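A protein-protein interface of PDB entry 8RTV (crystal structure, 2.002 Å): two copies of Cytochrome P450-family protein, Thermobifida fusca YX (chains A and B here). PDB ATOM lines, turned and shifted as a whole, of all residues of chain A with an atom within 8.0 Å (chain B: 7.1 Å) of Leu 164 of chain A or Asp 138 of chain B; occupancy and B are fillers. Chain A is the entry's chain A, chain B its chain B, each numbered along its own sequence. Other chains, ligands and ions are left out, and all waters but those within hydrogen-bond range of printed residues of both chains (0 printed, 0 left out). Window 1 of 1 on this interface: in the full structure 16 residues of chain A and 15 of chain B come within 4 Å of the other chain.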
ATOM      1  N   ALA A 141       2.409  12.141 -24.066  1.00  0.00           N
ATOM      2  CA  ALA A 141       3.551  12.962 -23.682  1.00  0.00           C
ATOM      3  C   ALA A 141       4.871  12.164 -23.680  1.00  0.00           C
ATOM      4  O   ALA A 141       5.875  12.700 -24.114  1.00  0.00           O
ATOM      5  CB  ALA A 141       3.264  13.610 -22.332  1.00  0.00           C
ATOM      6  N   PHE A 145       3.782  11.581 -28.957  1.00  0.00           N
ATOM      7  CA  PHE A 145       4.247  12.869 -29.449  1.00  0.00           C
ATOM      8  C   PHE A 145       5.755  12.870 -29.711  1.00  0.00           C
ATOM      9  O   PHE A 145       6.180  13.279 -30.779  1.00  0.00           O
ATOM     10  CB  PHE A 145       3.910  13.975 -28.448  1.00  0.00           C
ATOM     11  CG  PHE A 145       4.638  15.276 -28.736  1.00  0.00           C
ATOM     12  CD1 PHE A 145       4.415  15.941 -29.943  1.00  0.00           C
ATOM     13  CD2 PHE A 145       5.554  15.809 -27.812  1.00  0.00           C
ATOM     14  CE1 PHE A 145       5.103  17.119 -30.224  1.00  0.00           C
ATOM     15  CE2 PHE A 145       6.215  16.996 -28.071  1.00  0.00           C
ATOM     16  CZ  PHE A 145       5.987  17.655 -29.283  1.00  0.00           C
ATOM     17  N   ILE A 149       7.894  13.705 -33.621  1.00  0.00           N
ATOM     18  CA  ILE A 149       8.415  15.046 -33.758  1.00  0.00           C
ATOM     19  C   ILE A 149       9.950  14.977 -33.834  1.00  0.00           C
ATOM     20  O   ILE A 149      10.554  15.753 -34.575  1.00  0.00           O
ATOM     21  CB  ILE A 149       7.910  16.034 -32.681  1.00  0.00           C
ATOM     22  CG1 ILE A 149       8.239  17.448 -33.130  1.00  0.00           C
ATOM     23  CG2 ILE A 149       8.470  15.730 -31.289  1.00  0.00           C
ATOM     24  CD1 ILE A 149       7.441  18.540 -32.458  1.00  0.00           C
ATOM     25  N   ASN A 159      14.714  22.598 -34.312  1.00  0.00           N
ATOM     26  CA  ASN A 159      15.441  22.647 -33.041  1.00  0.00           C
ATOM     27  C   ASN A 159      14.543  22.177 -31.900  1.00  0.00           C
ATOM     28  O   ASN A 159      13.387  22.611 -31.756  1.00  0.00           O
ATOM     29  CB  ASN A 159      15.957  24.038 -32.689  1.00  0.00           C
ATOM     30  CG  ASN A 159      16.568  24.738 -33.885  1.00  0.00           C
ATOM     31  OD1 ASN A 159      16.146  25.843 -34.248  1.00  0.00           O
ATOM     32  ND2 ASN A 159      17.545  24.108 -34.511  1.00  0.00           N
ATOM     33  N   GLU A 160      15.117  21.303 -31.072  1.00  0.00           N
ATOM     34  CA  GLU A 160      14.423  20.693 -29.958  1.00  0.00           C
ATOM     35  C   GLU A 160      13.808  21.751 -29.042  1.00  0.00           C
ATOM     36  O   GLU A 160      12.803  21.493 -28.391  1.00  0.00           O
ATOM     37  CB  GLU A 160      15.424  19.813 -29.223  1.00  0.00           C
ATOM     38  CG  GLU A 160      14.744  18.898 -28.218  1.00  0.00           C
ATOM     39  CD  GLU A 160      15.690  18.415 -27.146  1.00  0.00           C
ATOM     40  OE1 GLU A 160      16.884  18.776 -27.165  1.00  0.00           O
ATOM     41  OE2 GLU A 160      15.181  17.673 -26.290  1.00  0.00           O
ATOM     42  N   GLU A 161      14.404  22.948 -29.018  1.00  0.00           N
ATOM     43  CA  GLU A 161      13.889  24.074 -28.261  1.00  0.00           C
ATOM     44  C   GLU A 161      12.487  24.510 -28.712  1.00  0.00           C
ATOM     45  O   GLU A 161      11.825  25.236 -27.986  1.00  0.00           O
ATOM     46  CB  GLU A 161      14.837  25.271 -28.370  1.00  0.00           C
ATOM     47  CG  GLU A 161      16.108  25.139 -27.544  1.00  0.00           C
ATOM     48  CD  GLU A 161      17.285  24.399 -28.168  1.00  0.00           C
ATOM     49  OE1 GLU A 161      17.207  23.771 -29.264  1.00  0.00           O
ATOM     50  OE2 GLU A 161      18.332  24.480 -27.483  1.00  0.00           O
ATOM     51  N   ASP A 162      12.067  24.136 -29.928  1.00  0.00           N
ATOM     52  CA  ASP A 162      10.823  24.615 -30.518  1.00  0.00           C
ATOM     53  C   ASP A 162       9.770  23.503 -30.544  1.00  0.00           C
ATOM     54  O   ASP A 162       8.643  23.735 -30.978  1.00  0.00           O
ATOM     55  CB  ASP A 162      11.063  25.143 -31.928  1.00  0.00           C
ATOM     56  CG  ASP A 162      12.082  26.271 -32.064  1.00  0.00           C
ATOM     57  OD1 ASP A 162      12.121  27.130 -31.165  1.00  0.00           O
ATOM     58  OD2 ASP A 162      12.805  26.295 -33.060  1.00  0.00           O
ATOM     59  N   HIS A 163      10.136  22.307 -30.070  1.00  0.00           N
ATOM     60  CA  HIS A 163       9.287  21.137 -30.235  1.00  0.00           C
ATOM     61  C   HIS A 163       7.928  21.340 -29.574  1.00  0.00           C
ATOM     62  O   HIS A 163       6.883  21.034 -30.158  1.00  0.00           O
ATOM     63  CB  HIS A 163       9.967  19.893 -29.671  1.00  0.00           C
ATOM     64  CG  HIS A 163      10.952  19.239 -30.568  1.00  0.00           C
ATOM     65  ND1 HIS A 163      11.490  18.021 -30.227  1.00  0.00           N
ATOM     66  CD2 HIS A 163      11.508  19.567 -31.741  1.00  0.00           C
ATOM     67  CE1 HIS A 163      12.339  17.636 -31.170  1.00  0.00           C
ATOM     68  NE2 HIS A 163      12.374  18.563 -32.096  1.00  0.00           N
ATOM     69  N   LEU A 164       7.964  21.821 -28.328  1.00  0.00           N
ATOM     70  CA  LEU A 164       6.749  22.053 -27.559  1.00  0.00           C
ATOM     71  C   LEU A 164       5.993  23.274 -28.084  1.00  0.00           C
ATOM     72  O   LEU A 164       4.759  23.271 -28.111  1.00  0.00           O
ATOM     73  CB  LEU A 164       7.080  22.155 -26.075  1.00  0.00           C
ATOM     74  CG  LEU A 164       7.594  20.847 -25.450  1.00  0.00           C
ATOM     75  CD1 LEU A 164       8.266  21.070 -24.082  1.00  0.00           C
ATOM     76  CD2 LEU A 164       6.446  19.853 -25.373  1.00  0.00           C
ATOM     77  N   THR A 165       6.720  24.303 -28.522  1.00  0.00           N
ATOM     78  CA  THR A 165       6.112  25.433 -29.211  1.00  0.00           C
ATOM     79  C   THR A 165       5.302  24.959 -30.419  1.00  0.00           C
ATOM     80  O   THR A 165       4.144  25.369 -30.594  1.00  0.00           O
ATOM     81  CB  THR A 165       7.201  26.388 -29.689  1.00  0.00           C
ATOM     82  OG1 THR A 165       7.865  26.775 -28.497  1.00  0.00           O
ATOM     83  CG2 THR A 165       6.647  27.600 -30.413  1.00  0.00           C
ATOM     84  N   LEU A 166       5.934  24.121 -31.257  1.00  0.00           N
ATOM     85  CA  LEU A 166       5.270  23.591 -32.432  1.00  0.00           C
ATOM     86  C   LEU A 166       4.036  22.747 -32.096  1.00  0.00           C
ATOM     87  O   LEU A 166       3.065  22.766 -32.858  1.00  0.00           O
ATOM     88  CB  LEU A 166       6.293  22.818 -33.261  1.00  0.00           C
ATOM     89  CG  LEU A 166       7.379  23.704 -33.880  1.00  0.00           C
ATOM     90  CD1 LEU A 166       8.391  22.812 -34.625  1.00  0.00           C
ATOM     91  CD2 LEU A 166       6.795  24.820 -34.756  1.00  0.00           C
ATOM     92  N   GLN A 167       4.055  22.008 -30.985  1.00  0.00           N
ATOM     93  CA  GLN A 167       2.948  21.136 -30.641  1.00  0.00           C
ATOM     94  C   GLN A 167       1.698  21.997 -30.467  1.00  0.00           C
ATOM     95  O   GLN A 167       0.617  21.676 -30.953  1.00  0.00           O
ATOM     96  CB  GLN A 167       3.274  20.368 -29.348  1.00  0.00           C
ATOM     97  CG  GLN A 167       2.229  19.310 -28.997  1.00  0.00           C
ATOM     98  CD  GLN A 167       2.560  18.551 -27.731  1.00  0.00           C
ATOM     99  OE1 GLN A 167       3.391  18.949 -26.904  1.00  0.00           O
ATOM    100  NE2 GLN A 167       1.881  17.439 -27.545  1.00  0.00           N
ATOM    101  N   THR A 168       1.863  23.120 -29.759  1.00  0.00           N
ATOM    102  CA  THR A 168       0.757  24.024 -29.492  1.00  0.00           C
ATOM    103  C   THR A 168       0.336  24.703 -30.793  1.00  0.00           C
ATOM    104  O   THR A 168      -0.843  24.831 -31.061  1.00  0.00           O
ATOM    105  CB  THR A 168       1.172  25.051 -28.433  1.00  0.00           C
ATOM    106  OG1 THR A 168       1.244  24.366 -27.185  1.00  0.00           O
ATOM    107  CG2 THR A 168       0.118  26.136 -28.277  1.00  0.00           C
ATOM    108  N   LEU A 169       1.314  25.108 -31.601  1.00  0.00           N
ATOM    109  CA  LEU A 169       1.052  25.892 -32.798  1.00  0.00           C
ATOM    110  C   LEU A 169       0.207  25.074 -33.781  1.00  0.00           C
ATOM    111  O   LEU A 169      -0.784  25.573 -34.323  1.00  0.00           O
ATOM    112  CB  LEU A 169       2.421  26.250 -33.375  1.00  0.00           C
ATOM    113  CG  LEU A 169       2.654  27.719 -33.737  1.00  0.00           C
ATOM    114  CD1 LEU A 169       2.253  28.717 -32.657  1.00  0.00           C
ATOM    115  CD2 LEU A 169       4.124  27.900 -34.042  1.00  0.00           C
ATOM    116  N   VAL A 170       0.569  23.789 -33.943  1.00  0.00           N
ATOM    117  CA  VAL A 170      -0.133  22.881 -34.843  1.00  0.00           C
ATOM    118  C   VAL A 170      -1.548  22.620 -34.327  1.00  0.00           C
ATOM    119  O   VAL A 170      -2.522  22.675 -35.069  1.00  0.00           O
ATOM    120  CB  VAL A 170       0.680  21.586 -34.983  1.00  0.00           C
ATOM    121  CG1 VAL A 170      -0.094  20.478 -35.686  1.00  0.00           C
ATOM    122  CG2 VAL A 170       1.989  21.848 -35.679  1.00  0.00           C
ATOM    123  N   THR A 171      -1.672  22.331 -33.038  1.00  0.00           N
ATOM    124  CA  THR A 171      -2.997  22.136 -32.460  1.00  0.00           C
ATOM    125  C   THR A 171      -3.874  23.363 -32.758  1.00  0.00           C
ATOM    126  O   THR A 171      -5.056  23.211 -33.070  1.00  0.00           O
ATOM    127  CB  THR A 171      -2.892  21.873 -30.955  1.00  0.00           C
ATOM    128  OG1 THR A 171      -1.995  20.785 -30.733  1.00  0.00           O
ATOM    129  CG2 THR A 171      -4.244  21.595 -30.320  1.00  0.00           C
ATOM    130  N   PHE A 188       5.934  32.558 -36.807  1.00  0.00           N
ATOM    131  CA  PHE A 188       6.867  31.675 -36.136  1.00  0.00           C
ATOM    132  C   PHE A 188       7.779  31.040 -37.175  1.00  0.00           C
ATOM    133  O   PHE A 188       8.999  31.060 -37.019  1.00  0.00           O
ATOM    134  CB  PHE A 188       6.199  30.606 -35.271  1.00  0.00           C
ATOM    135  CG  PHE A 188       7.249  29.803 -34.536  1.00  0.00           C
ATOM    136  CD1 PHE A 188       7.809  30.289 -33.356  1.00  0.00           C
ATOM    137  CD2 PHE A 188       7.725  28.604 -35.056  1.00  0.00           C
ATOM    138  CE1 PHE A 188       8.776  29.550 -32.686  1.00  0.00           C
ATOM    139  CE2 PHE A 188       8.686  27.875 -34.375  1.00  0.00           C
ATOM    140  CZ  PHE A 188       9.224  28.353 -33.212  1.00  0.00           C
ATOM    141  N   PHE A 236       4.143  15.451 -37.716  1.00  0.00           N
ATOM    142  CA  PHE A 236       4.119  14.693 -36.463  1.00  0.00           C
ATOM    143  C   PHE A 236       2.700  14.474 -35.919  1.00  0.00           C
ATOM    144  O   PHE A 236       2.456  13.436 -35.297  1.00  0.00           O
ATOM    145  CB  PHE A 236       5.034  15.294 -35.378  1.00  0.00           C
ATOM    146  CG  PHE A 236       4.599  16.666 -34.870  1.00  0.00           C
ATOM    147  CD1 PHE A 236       3.616  16.787 -33.880  1.00  0.00           C
ATOM    148  CD2 PHE A 236       5.160  17.824 -35.379  1.00  0.00           C
ATOM    149  CE1 PHE A 236       3.200  18.031 -33.438  1.00  0.00           C
ATOM    150  CE2 PHE A 236       4.745  19.070 -34.936  1.00  0.00           C
ATOM    151  CZ  PHE A 236       3.751  19.166 -33.993  1.00  0.00           C
ATOM    152  N   MET B 130      13.501  14.044 -13.001  1.00  0.00           N
ATOM    153  CA  MET B 130      13.959  15.053 -13.953  1.00  0.00           C
ATOM    154  C   MET B 130      15.441  14.864 -14.262  1.00  0.00           C
ATOM    155  O   MET B 130      15.863  15.142 -15.380  1.00  0.00           O
ATOM    156  CB  MET B 130      13.707  16.478 -13.440  1.00  0.00           C
ATOM    157  CG  MET B 130      12.214  16.777 -13.305  1.00  0.00           C
ATOM    158  SD  MET B 130      11.823  18.241 -12.329  1.00  0.00           S
ATOM    159  CE  MET B 130      12.788  19.523 -13.140  1.00  0.00           C
ATOM    160  N   GLY B 135      17.434  16.299 -22.548  1.00  0.00           N
ATOM    161  CA  GLY B 135      17.381  17.550 -23.297  1.00  0.00           C
ATOM    162  C   GLY B 135      16.268  18.462 -22.782  1.00  0.00           C
ATOM    163  O   GLY B 135      16.112  18.621 -21.587  1.00  0.00           O
ATOM    164  N   VAL B 136      15.473  19.040 -23.681  1.00  0.00           N
ATOM    165  CA  VAL B 136      14.415  19.966 -23.286  1.00  0.00           C
ATOM    166  C   VAL B 136      13.352  19.197 -22.491  1.00  0.00           C
ATOM    167  O   VAL B 136      13.051  18.058 -22.811  1.00  0.00           O
ATOM    168  CB  VAL B 136      13.824  20.705 -24.507  1.00  0.00           C
ATOM    169  CG1 VAL B 136      12.639  21.618 -24.150  1.00  0.00           C
ATOM    170  CG2 VAL B 136      14.915  21.503 -25.209  1.00  0.00           C
ATOM    171  N   VAL B 137      12.803  19.834 -21.450  1.00  0.00           N
ATOM    172  CA  VAL B 137      11.800  19.244 -20.565  1.00  0.00           C
ATOM    173  C   VAL B 137      10.662  20.250 -20.369  1.00  0.00           C
ATOM    174  O   VAL B 137      10.890  21.449 -20.205  1.00  0.00           O
ATOM    175  CB  VAL B 137      12.485  18.860 -19.231  1.00  0.00           C
ATOM    176  CG1 VAL B 137      11.604  19.032 -17.994  1.00  0.00           C
ATOM    177  CG2 VAL B 137      13.083  17.459 -19.294  1.00  0.00           C
ATOM    178  N   ASP B 138       9.421  19.762 -20.379  1.00  0.00           N
ATOM    179  CA  ASP B 138       8.292  20.584 -19.991  1.00  0.00           C
ATOM    180  C   ASP B 138       8.215  20.605 -18.462  1.00  0.00           C
ATOM    181  O   ASP B 138       7.760  19.629 -17.849  1.00  0.00           O
ATOM    182  CB  ASP B 138       6.983  20.099 -20.608  1.00  0.00           C
ATOM    183  CG  ASP B 138       5.794  20.988 -20.269  1.00  0.00           C
ATOM    184  OD1 ASP B 138       6.000  22.089 -19.682  1.00  0.00           O
ATOM    185  OD2 ASP B 138       4.665  20.564 -20.558  1.00  0.00           O
ATOM    186  N   LEU B 139       8.616  21.738 -17.872  1.00  0.00           N
ATOM    187  CA  LEU B 139       8.590  21.923 -16.423  1.00  0.00           C
ATOM    188  C   LEU B 139       7.182  21.724 -15.845  1.00  0.00           C
ATOM    189  O   LEU B 139       7.039  21.183 -14.750  1.00  0.00           O
ATOM    190  CB  LEU B 139       9.114  23.295 -16.034  1.00  0.00           C
ATOM    191  CG  LEU B 139       9.310  23.513 -14.531  1.00  0.00           C
ATOM    192  CD1 LEU B 139      10.456  22.695 -13.947  1.00  0.00           C
ATOM    193  CD2 LEU B 139       9.523  24.983 -14.262  1.00  0.00           C
ATOM    194  N   LYS B 140       6.152  22.108 -16.600  1.00  0.00           N
ATOM    195  CA  LYS B 140       4.783  21.960 -16.145  1.00  0.00           C
ATOM    196  C   LYS B 140       4.476  20.480 -15.918  1.00  0.00           C
ATOM    197  O   LYS B 140       4.161  20.088 -14.812  1.00  0.00           O
ATOM    198  CB  LYS B 140       3.777  22.559 -17.130  1.00  0.00           C
ATOM    199  CG  LYS B 140       2.344  22.510 -16.621  1.00  0.00           C
ATOM    200  CD  LYS B 140       1.322  23.000 -17.616  1.00  0.00           C
ATOM    201  CE  LYS B 140      -0.041  22.571 -17.199  1.00  0.00           C
ATOM    202  NZ  LYS B 140      -1.069  23.484 -17.682  1.00  0.00           N
ATOM    203  N   ALA B 141       4.663  19.655 -16.950  1.00  0.00           N
ATOM    204  CA  ALA B 141       4.406  18.220 -16.912  1.00  0.00           C
ATOM    205  C   ALA B 141       5.288  17.471 -15.911  1.00  0.00           C
ATOM    206  O   ALA B 141       4.786  16.563 -15.233  1.00  0.00           O
ATOM    207  CB  ALA B 141       4.531  17.656 -18.326  1.00  0.00           C
ATOM    208  N   ALA B 142       6.584  17.827 -15.830  1.00  0.00           N
ATOM    209  CA  ALA B 142       7.548  17.175 -14.942  1.00  0.00           C
ATOM    210  C   ALA B 142       7.476  17.618 -13.475  1.00  0.00           C
ATOM    211  O   ALA B 142       7.974  16.914 -12.581  1.00  0.00           O
ATOM    212  CB  ALA B 142       8.977  17.475 -15.428  1.00  0.00           C
ATOM    213  N   TYR B 143       7.032  18.858 -13.207  1.00  0.00           N
ATOM    214  CA  TYR B 143       7.299  19.439 -11.902  1.00  0.00           C
ATOM    215  C   TYR B 143       6.097  20.188 -11.353  1.00  0.00           C
ATOM    216  O   TYR B 143       5.587  19.781 -10.315  1.00  0.00           O
ATOM    217  CB  TYR B 143       8.539  20.320 -11.986  1.00  0.00           C
ATOM    218  CG  TYR B 143       9.135  20.667 -10.629  1.00  0.00           C
ATOM    219  CD1 TYR B 143       9.700  19.672  -9.826  1.00  0.00           C
ATOM    220  CD2 TYR B 143       9.165  21.982 -10.159  1.00  0.00           C
ATOM    221  CE1 TYR B 143      10.250  19.966  -8.585  1.00  0.00           C
ATOM    222  CE2 TYR B 143       9.741  22.295  -8.931  1.00  0.00           C
ATOM    223  CZ  TYR B 143      10.277  21.283  -8.140  1.00  0.00           C
ATOM    224  OH  TYR B 143      10.875  21.550  -6.934  1.00  0.00           O
ATOM    225  N   SER B 144       5.664  21.238 -12.069  1.00  0.00           N
ATOM    226  CA  SER B 144       4.705  22.206 -11.598  1.00  0.00           C
ATOM    227  C   SER B 144       3.360  21.548 -11.351  1.00  0.00           C
ATOM    228  O   SER B 144       2.692  21.932 -10.412  1.00  0.00           O
ATOM    229  CB  SER B 144       4.525  23.354 -12.583  1.00  0.00           C
ATOM    230  OG  SER B 144       5.783  23.885 -12.951  1.00  0.00           O
ATOM    231  N   SER B 244       5.288  27.594 -12.223  1.00  0.00           N
ATOM    232  CA  SER B 244       5.790  28.004 -13.522  1.00  0.00           C
ATOM    233  C   SER B 244       5.985  29.515 -13.597  1.00  0.00           C
ATOM    234  O   SER B 244       7.021  29.970 -14.048  1.00  0.00           O
ATOM    235  CB  SER B 244       4.896  27.507 -14.646  1.00  0.00           C
ATOM    236  OG  SER B 244       4.990  26.104 -14.730  1.00  0.00           O
ATOM    237  N   GLY B 373      12.255  28.093 -25.544  1.00  0.00           N
ATOM    238  CA  GLY B 373      11.053  27.993 -26.339  1.00  0.00           C
ATOM    239  C   GLY B 373      10.065  29.074 -25.939  1.00  0.00           C
ATOM    240  O   GLY B 373      10.425  30.117 -25.406  1.00  0.00           O
ATOM    241  N   GLU B 374       8.804  28.749 -26.150  1.00  0.00           N
ATOM    242  CA  GLU B 374       7.692  29.613 -25.834  1.00  0.00           C
ATOM    243  C   GLU B 374       6.864  28.911 -24.776  1.00  0.00           C
ATOM    244  O   GLU B 374       6.897  27.689 -24.655  1.00  0.00           O
ATOM    245  CB  GLU B 374       6.864  29.852 -27.093  1.00  0.00           C
ATOM    246  CG  GLU B 374       7.637  30.648 -28.138  1.00  0.00           C
ATOM    247  CD  GLU B 374       6.806  31.160 -29.309  1.00  0.00           C
ATOM    248  OE1 GLU B 374       5.554  31.061 -29.281  1.00  0.00           O
ATOM    249  OE2 GLU B 374       7.433  31.663 -30.264  1.00  0.00           O
ATOM    250  N   PRO B 376       3.100  29.398 -24.244  1.00  0.00           N
ATOM    251  CA  PRO B 376       1.825  30.009 -24.591  1.00  0.00           C
ATOM    252  C   PRO B 376       0.865  29.936 -23.405  1.00  0.00           C
ATOM    253  O   PRO B 376       0.888  28.978 -22.627  1.00  0.00           O
ATOM    254  CB  PRO B 376       1.384  29.146 -25.788  1.00  0.00           C
ATOM    255  CG  PRO B 376       1.965  27.778 -25.471  1.00  0.00           C
ATOM    256  CD  PRO B 376       3.342  28.129 -24.939  1.00  0.00           C
ATOM    257  N   PRO B 386       0.932  29.166 -17.945  1.00  0.00           N
ATOM    258  CA  PRO B 386       1.200  28.613 -19.270  1.00  0.00           C
ATOM    259  C   PRO B 386       0.700  27.189 -19.531  1.00  0.00           C
ATOM    260  O   PRO B 386       0.594  26.375 -18.614  1.00  0.00           O
ATOM    261  CB  PRO B 386       2.731  28.730 -19.352  1.00  0.00           C
ATOM    262  CG  PRO B 386       3.215  28.609 -17.917  1.00  0.00           C
ATOM    263  CD  PRO B 386       2.103  29.183 -17.045  1.00  0.00           C
ATOM    264  N   LEU B 387       0.413  26.908 -20.814  1.00  0.00           N
ATOM    265  CA  LEU B 387       0.051  25.573 -21.270  1.00  0.00           C
ATOM    266  C   LEU B 387       1.238  24.623 -21.114  1.00  0.00           C
ATOM    267  O   LEU B 387       1.048  23.439 -20.859  1.00  0.00           O
ATOM    268  CB  LEU B 387      -0.371  25.597 -22.741  1.00  0.00           C
ATOM    269  CG  LEU B 387      -1.803  26.005 -23.065  1.00  0.00           C
ATOM    270  CD1 LEU B 387      -1.974  25.957 -24.590  1.00  0.00           C
ATOM    271  CD2 LEU B 387      -2.836  25.141 -22.351  1.00  0.00           C
ATOM    272  N   SER B 388       2.453  25.154 -21.335  1.00  0.00           N
ATOM    273  CA  SER B 388       3.686  24.401 -21.190  1.00  0.00           C
ATOM    274  C   SER B 388       4.791  25.344 -20.723  1.00  0.00           C
ATOM    275  O   SER B 388       4.669  26.548 -20.899  1.00  0.00           O
ATOM    276  CB  SER B 388       4.045  23.742 -22.500  1.00  0.00           C
ATOM    277  OG  SER B 388       4.359  24.738 -23.464  1.00  0.00           O
ATOM    278  N   ARG B 389       5.859  24.805 -20.123  1.00  0.00           N
ATOM    279  CA  ARG B 389       6.966  25.653 -19.688  1.00  0.00           C
ATOM    280  C   ARG B 389       8.280  24.951 -20.020  1.00  0.00           C
ATOM    281  O   ARG B 389       8.920  24.387 -19.129  1.00  0.00           O
ATOM    282  CB  ARG B 389       6.892  26.051 -18.205  1.00  0.00           C
ATOM    283  CG  ARG B 389       7.931  27.048 -17.714  1.00  0.00           C
ATOM    284  CD  ARG B 389       9.150  27.385 -18.623  1.00  0.00           C
ATOM    285  NE  ARG B 389       8.678  28.465 -19.482  1.00  0.00           N
ATOM    286  CZ  ARG B 389       9.253  29.248 -20.368  1.00  0.00           C
ATOM    287  NH1 ARG B 389      10.190  28.865 -21.223  1.00  0.00           N
ATOM    288  NH2 ARG B 389       8.775  30.474 -20.427  1.00  0.00           N
ATOM    289  N   PRO B 390       8.747  25.024 -21.288  1.00  0.00           N
ATOM    290  CA  PRO B 390       9.971  24.321 -21.696  1.00  0.00           C
ATOM    291  C   PRO B 390      11.186  24.876 -20.980  1.00  0.00           C
ATOM    292  O   PRO B 390      11.353  26.095 -20.914  1.00  0.00           O
ATOM    293  CB  PRO B 390      10.068  24.555 -23.193  1.00  0.00           C
ATOM    294  CG  PRO B 390       8.666  24.981 -23.588  1.00  0.00           C
ATOM    295  CD  PRO B 390       8.131  25.791 -22.387  1.00  0.00           C
ATOM    296  N   VAL B 391      12.003  23.971 -20.435  1.00  0.00           N
ATOM    297  CA  VAL B 391      13.275  24.373 -19.835  1.00  0.00           C
ATOM    298  C   VAL B 391      14.383  23.419 -20.287  1.00  0.00           C
ATOM    299  O   VAL B 391      14.110  22.308 -20.736  1.00  0.00           O
ATOM    300  CB  VAL B 391      13.191  24.408 -18.305  1.00  0.00           C
ATOM    301  CG1 VAL B 391      12.127  25.403 -17.818  1.00  0.00           C
ATOM    302  CG2 VAL B 391      12.965  22.996 -17.747  1.00  0.00           C
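Among the printed residues, merely in contact across the chains: Glu 160 of chain A with Gly 135 of chain B (3.7 Å), Glu 161 of chain A with Gly 373 of chain B (3.3 Å), Leu 164 of chain A with Asp 138 of chain B (3.8 Å), Leu 164 of chain A with Pro 390 of chain B (3.96 Å), Thr 168 of chain A with Pro 376 of chain B (3.7 Å) and Phe 188 of chain A with Glu 374 of chain B (3.4 Å).
1 position is printed for both chains.
The side-chain hydroxyl of Thr 165 of chain A lies within hydrogen-bond range of the backbone NH of Glu 374 of chain B, 3.2 Å away.
The side-chain carboxylate (OE2) of Glu 160 of chain A is in hydrogen-bond range of the backbone NH (N) of Val 136 of chain B, 3.0 Å away.
Of chain A, only Leu 164 (3.8 Å) comes within 4 Å of Asp 138 of chain B.
Of the printed residues of chain B, Thr 165 of chain A touches Glu 374 (3.2 Å).
Of the printed residues of chain A, Glu 374 of chain B touches Thr 165 (3.2 Å) and Phe 188 (3.4 Å).
Ala 141 of chain B touches none of the printed residues of chain A.
The nearest residue of chain B that does not touch Leu 164 of chain A is Val 136 of chain B (4.4 Å).
The side-chain carboxylate (OD1) of Asp 138 of chain B lies within hydrogen-bond range of the backbone NH (N) of Lys 140 of chain B.
The backbone NH of Arg 389 of chain B is in hydrogen-bond range of the side-chain carboxylate of Asp 138 of chain B, 2.8 Å away.
O of Pro 376 of chain B lies within hydrogen-bond range of N of Leu 387 of chain B.
Printed residues of chain A that touch a printed residue of chain B: Glu 160, Glu 161, Leu 164, Thr 165, Thr 168 and Phe 188.
Hydrophobic or aromatic side chains of chain B within 4 Å of the printed part of chain A: Val 136, Pro 376 and Pro 390.
Among the printed residues, 8 pairs touch across the chains.
Among the printed residues, no Asp or Glu carboxylate lies within 4 Å of a Lys or Arg side-chain nitrogen of the other chain.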
